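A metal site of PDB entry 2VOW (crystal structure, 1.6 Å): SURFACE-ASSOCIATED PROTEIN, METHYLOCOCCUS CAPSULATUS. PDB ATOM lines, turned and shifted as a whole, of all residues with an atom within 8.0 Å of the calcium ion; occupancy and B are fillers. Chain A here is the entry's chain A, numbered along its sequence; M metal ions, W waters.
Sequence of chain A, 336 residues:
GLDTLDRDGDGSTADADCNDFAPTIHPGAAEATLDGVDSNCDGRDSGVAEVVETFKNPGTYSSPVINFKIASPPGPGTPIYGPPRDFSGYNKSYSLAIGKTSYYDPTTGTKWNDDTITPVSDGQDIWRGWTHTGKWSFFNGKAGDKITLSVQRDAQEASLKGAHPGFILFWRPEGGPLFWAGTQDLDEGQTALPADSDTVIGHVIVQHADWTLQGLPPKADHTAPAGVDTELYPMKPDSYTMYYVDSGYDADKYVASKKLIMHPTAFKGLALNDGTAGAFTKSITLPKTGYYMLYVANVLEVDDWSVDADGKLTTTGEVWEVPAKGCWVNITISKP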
ATOM      1  N   VAL A 151       4.330 -33.874  15.448  1.00  0.00           N
ATOM      2  CA  VAL A 151       3.020 -34.489  15.245  1.00  0.00           C
ATOM      3  C   VAL A 151       2.354 -33.749  14.110  1.00  0.00           C
ATOM      4  O   VAL A 151       2.308 -32.530  14.114  1.00  0.00           O
ATOM      5  CB  VAL A 151       2.099 -34.470  16.485  1.00  0.00           C
ATOM      6  CG1 VAL A 151       0.789 -35.259  16.185  1.00  0.00           C
ATOM      7  CG2 VAL A 151       2.829 -35.062  17.709  1.00  0.00           C
ATOM      8  N   ALA A 163      -7.189 -31.573  12.428  1.00  0.00           N
ATOM      9  CA  ALA A 163      -6.157 -31.737  13.441  1.00  0.00           C
ATOM     10  C   ALA A 163      -5.535 -30.406  13.875  1.00  0.00           C
ATOM     11  O   ALA A 163      -5.207 -29.561  13.031  1.00  0.00           O
ATOM     12  CB  ALA A 163      -5.053 -32.681  12.913  1.00  0.00           C
ATOM     13  N   HIS A 164      -5.393 -30.241  15.186  1.00  0.00           N
ATOM     14  CA  HIS A 164      -4.456 -29.284  15.793  1.00  0.00           C
ATOM     15  C   HIS A 164      -3.831 -30.053  16.966  1.00  0.00           C
ATOM     16  O   HIS A 164      -4.271 -29.944  18.111  1.00  0.00           O
ATOM     17  CB  HIS A 164      -5.126 -28.022  16.325  1.00  0.00           C
ATOM     18  CG  HIS A 164      -5.661 -27.105  15.258  1.00  0.00           C
ATOM     19  ND1 HIS A 164      -4.855 -26.401  14.392  1.00  0.00           N
ATOM     20  CD2 HIS A 164      -6.938 -26.760  14.961  1.00  0.00           C
ATOM     21  CE1 HIS A 164      -5.616 -25.649  13.606  1.00  0.00           C
ATOM     22  NE2 HIS A 164      -6.877 -25.849  13.931  1.00  0.00           N
ATOM     23  N   PRO A 165      -2.833 -30.879  16.664  1.00  0.00           N
ATOM     24  CA  PRO A 165      -2.324 -31.770  17.734  1.00  0.00           C
ATOM     25  C   PRO A 165      -1.652 -31.011  18.862  1.00  0.00           C
ATOM     26  O   PRO A 165      -1.053 -29.955  18.638  1.00  0.00           O
ATOM     27  CB  PRO A 165      -1.272 -32.620  17.027  1.00  0.00           C
ATOM     28  CG  PRO A 165      -1.083 -32.043  15.674  1.00  0.00           C
ATOM     29  CD  PRO A 165      -2.171 -31.090  15.365  1.00  0.00           C
ATOM     30  N   TYR A 249       0.917 -27.154  21.793  1.00  0.00           N
ATOM     31  CA  TYR A 249      -0.124 -27.535  20.827  1.00  0.00           C
ATOM     32  C   TYR A 249       0.001 -26.651  19.605  1.00  0.00           C
ATOM     33  O   TYR A 249       0.518 -25.524  19.677  1.00  0.00           O
ATOM     34  CB  TYR A 249      -1.534 -27.427  21.438  1.00  0.00           C
ATOM     35  CG  TYR A 249      -1.933 -25.994  21.736  1.00  0.00           C
ATOM     36  CD1 TYR A 249      -2.633 -25.232  20.798  1.00  0.00           C
ATOM     37  CD2 TYR A 249      -1.565 -25.400  22.955  1.00  0.00           C
ATOM     38  CE1 TYR A 249      -2.972 -23.903  21.063  1.00  0.00           C
ATOM     39  CE2 TYR A 249      -1.897 -24.056  23.216  1.00  0.00           C
ATOM     40  CZ  TYR A 249      -2.584 -23.313  22.275  1.00  0.00           C
ATOM     41  OH  TYR A 249      -2.925 -21.993  22.552  1.00  0.00           O
ATOM     42  N   ASP A 250      -0.418 -27.205  18.480  1.00  0.00           N
ATOM     43  CA  ASP A 250      -0.522 -26.486  17.230  1.00  0.00           C
ATOM     44  C   ASP A 250      -1.545 -25.359  17.323  1.00  0.00           C
ATOM     45  O   ASP A 250      -2.746 -25.597  17.363  1.00  0.00           O
ATOM     46  CB  ASP A 250      -0.947 -27.466  16.137  1.00  0.00           C
ATOM     47  CG  ASP A 250      -1.185 -26.776  14.836  1.00  0.00           C
ATOM     48  OD1 ASP A 250      -0.402 -25.847  14.520  1.00  0.00           O
ATOM     49  OD2 ASP A 250      -2.156 -27.128  14.173  1.00  0.00           O
ATOM     50  N   ALA A 251      -1.055 -24.126  17.268  1.00  0.00           N
ATOM     51  CA  ALA A 251      -1.894 -22.919  17.393  1.00  0.00           C
ATOM     52  C   ALA A 251      -2.145 -22.219  16.058  1.00  0.00           C
ATOM     53  O   ALA A 251      -2.815 -21.162  16.031  1.00  0.00           O
ATOM     54  CB  ALA A 251      -1.251 -21.953  18.383  1.00  0.00           C
ATOM     55  N   ASP A 252      -1.618 -22.779  14.979  1.00  0.00           N
ATOM     56  CA  ASP A 252      -1.835 -22.246  13.630  1.00  0.00           C
ATOM     57  C   ASP A 252      -3.215 -22.626  13.142  1.00  0.00           C
ATOM     58  O   ASP A 252      -3.502 -23.792  12.877  1.00  0.00           O
ATOM     59  CB  ASP A 252      -0.762 -22.807  12.688  1.00  0.00           C
ATOM     60  CG  ASP A 252       0.638 -22.403  13.108  1.00  0.00           C
ATOM     61  OD1 ASP A 252       0.982 -21.198  13.038  1.00  0.00           O
ATOM     62  OD2 ASP A 252       1.397 -23.295  13.517  1.00  0.00           O
ATOM     63  N   LYS A 253      -4.101 -21.639  13.028  1.00  0.00           N
ATOM     64  CA  LYS A 253      -5.467 -21.870  12.562  1.00  0.00           C
ATOM     65  C   LYS A 253      -5.606 -22.170  11.067  1.00  0.00           C
ATOM     66  O   LYS A 253      -4.845 -21.648  10.245  1.00  0.00           O
ATOM     67  CB  LYS A 253      -6.365 -20.694  12.953  1.00  0.00           C
ATOM     68  CG  LYS A 253      -6.583 -20.554  14.455  1.00  0.00           C
ATOM     69  CD  LYS A 253      -7.553 -19.407  14.792  1.00  0.00           C
ATOM     70  CE  LYS A 253      -6.831 -18.047  14.709  1.00  0.00           C
ATOM     71  NZ  LYS A 253      -7.768 -16.918  14.985  1.00  0.00           N
ATOM     72  N   LEU A 272       2.244 -23.160  19.929  1.00  0.00           N
ATOM     73  CA  LEU A 272       3.313 -23.354  18.960  1.00  0.00           C
ATOM     74  C   LEU A 272       2.809 -22.871  17.604  1.00  0.00           C
ATOM     75  O   LEU A 272       1.807 -23.361  17.101  1.00  0.00           O
ATOM     76  CB  LEU A 272       3.734 -24.832  18.883  1.00  0.00           C
ATOM     77  CG  LEU A 272       4.353 -25.443  20.156  1.00  0.00           C
ATOM     78  CD1 LEU A 272       4.450 -26.943  20.031  1.00  0.00           C
ATOM     79  CD2 LEU A 272       5.755 -24.856  20.493  1.00  0.00           C
ATOM     80  N   ASN A 273       3.480 -21.867  17.039  1.00  0.00           N
ATOM     81  CA  ASN A 273       3.122 -21.359  15.715  1.00  0.00           C
ATOM     82  C   ASN A 273       4.281 -21.543  14.750  1.00  0.00           C
ATOM     83  O   ASN A 273       5.392 -21.054  14.992  1.00  0.00           O
ATOM     84  CB  ASN A 273       2.712 -19.881  15.756  1.00  0.00           C
ATOM     85  CG  ASN A 273       1.392 -19.664  16.482  1.00  0.00           C
ATOM     86  OD1 ASN A 273       0.306 -19.779  15.897  1.00  0.00           O
ATOM     87  ND2 ASN A 273       1.487 -19.348  17.754  1.00  0.00           N
ATOM     88  N   ASP A 274       4.037 -22.269  13.662  1.00  0.00           N
ATOM     89  CA  ASP A 274       5.046 -22.481  12.623  1.00  0.00           C
ATOM     90  C   ASP A 274       4.473 -22.204  11.240  1.00  0.00           C
ATOM     91  O   ASP A 274       5.099 -22.555  10.245  1.00  0.00           O
ATOM     92  CB  ASP A 274       5.679 -23.878  12.699  1.00  0.00           C
ATOM     93  CG  ASP A 274       4.642 -25.009  12.623  1.00  0.00           C
ATOM     94  OD1 ASP A 274       3.504 -24.783  12.127  1.00  0.00           O
ATOM     95  OD2 ASP A 274       4.996 -26.140  13.055  1.00  0.00           O
ATOM     96  N   GLY A 275       3.288 -21.592  11.186  1.00  0.00           N
ATOM     97  CA  GLY A 275       2.633 -21.245   9.930  1.00  0.00           C
ATOM     98  C   GLY A 275       1.940 -22.401   9.228  1.00  0.00           C
ATOM     99  O   GLY A 275       1.366 -22.225   8.152  1.00  0.00           O
ATOM    100  N   THR A 276       1.993 -23.587   9.850  1.00  0.00           N
ATOM    101  CA  THR A 276       1.383 -24.793   9.278  1.00  0.00           C
ATOM    102  C   THR A 276       0.313 -25.320  10.227  1.00  0.00           C
ATOM    103  O   THR A 276       0.656 -25.781  11.324  1.00  0.00           O
ATOM    104  CB  THR A 276       2.437 -25.901   8.994  1.00  0.00           C
ATOM    105  OG1 THR A 276       3.351 -25.466   7.964  1.00  0.00           O
ATOM    106  CG2 THR A 276       1.774 -27.199   8.548  1.00  0.00           C
ATOM    107  N   ALA A 277      -0.947 -25.195   9.811  1.00  0.00           N
ATOM    108  CA  ALA A 277      -2.088 -25.756  10.556  1.00  0.00           C
ATOM    109  C   ALA A 277      -2.064 -27.263  10.432  1.00  0.00           C
ATOM    110  O   ALA A 277      -1.798 -27.800   9.348  1.00  0.00           O
ATOM    111  CB  ALA A 277      -3.370 -25.229   9.995  1.00  0.00           C
ATOM    112  N   GLY A 278      -2.338 -27.934  11.545  1.00  0.00           N
ATOM    113  CA  GLY A 278      -2.395 -29.377  11.582  1.00  0.00           C
ATOM    114  C   GLY A 278      -1.131 -30.108  11.980  1.00  0.00           C
ATOM    115  O   GLY A 278      -1.113 -31.337  11.971  1.00  0.00           O
ATOM    116  N   ALA A 279      -0.074 -29.359  12.337  1.00  0.00           N
ATOM    117  CA  ALA A 279       1.232 -29.937  12.629  1.00  0.00           C
ATOM    118  C   ALA A 279       1.964 -29.073  13.645  1.00  0.00           C
ATOM    119  O   ALA A 279       1.809 -27.836  13.643  1.00  0.00           O
ATOM    120  CB  ALA A 279       2.063 -30.047  11.347  1.00  0.00           C
ATOM    121  N   PHE A 280       2.730 -29.694  14.539  1.00  0.00           N
ATOM    122  CA  PHE A 280       3.752 -28.948  15.304  1.00  0.00           C
ATOM    123  C   PHE A 280       5.060 -29.742  15.373  1.00  0.00           C
ATOM    124  O   PHE A 280       5.082 -30.950  15.138  1.00  0.00           O
ATOM    125  CB  PHE A 280       3.261 -28.568  16.721  1.00  0.00           C
ATOM    126  CG  PHE A 280       3.257 -29.722  17.681  1.00  0.00           C
ATOM    127  CD1 PHE A 280       4.436 -30.112  18.325  1.00  0.00           C
ATOM    128  CD2 PHE A 280       2.078 -30.473  17.887  1.00  0.00           C
ATOM    129  CE1 PHE A 280       4.455 -31.233  19.206  1.00  0.00           C
ATOM    130  CE2 PHE A 280       2.078 -31.566  18.766  1.00  0.00           C
ATOM    131  CZ  PHE A 280       3.261 -31.962  19.398  1.00  0.00           C
ATOM    132  N   THR A 281       6.137 -29.032  15.713  1.00  0.00           N
ATOM    133  CA  THR A 281       7.435 -29.611  16.011  1.00  0.00           C
ATOM    134  C   THR A 281       7.973 -28.879  17.239  1.00  0.00           C
ATOM    135  O   THR A 281       7.770 -27.656  17.371  1.00  0.00           O
ATOM    136  CB  THR A 281       8.401 -29.465  14.806  1.00  0.00           C
ATOM    137  OG1 THR A 281       7.790 -30.004  13.631  1.00  0.00           O
ATOM    138  CG2 THR A 281       9.667 -30.213  15.050  1.00  0.00           C
HETATM  139 CA    CA M   1       1.629 -25.602  13.310  1.00  0.00          CA
HETATM  140  O   HOH W   1       2.745 -25.421  15.402  1.00  0.00           O
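The backbone NH of Gly 275 sits at hydrogen-bond distance from the side-chain carboxylate of Asp 252. OD1 of Asn 273 lies close to OD1 of Asp 252, at 3.3 Å. O of Asp 252 lies close to ND1 of His 164 (3.3 Å). OD2 of Asp 250 is in hydrogen-bond range of N of Gly 278. ND1 of His 164 lies within hydrogen-bond range of OD2 of Asp 250 (2.8 Å). The backbone carbonyl oxygen (O) of Pro 165 lies within hydrogen-bond range of the backbone NH (N) of Asp 250, at 2.8 Å.
The calcium ion is bound by the backbone carbonyl oxygen of Thr 276 (2.2 Å), the backbone carbonyl oxygen of Ala 279 (2.3 Å), the side-chain carboxylate of Asp 252 (2.3 Å), the side-chain carboxylate of Asp 274 (2.4 Å), the side-chain carboxylate of Asp 250 (2.4 Å) and water W1 (2.4 Å). The calcium ion has six donor atoms within binding distance.
Water W1 lies within hydrogen-bond range of the backbone carbonyl oxygen of Leu 272 (2.8 Å) and the side-chain carboxylate of Asp 274 (3.3 Å).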
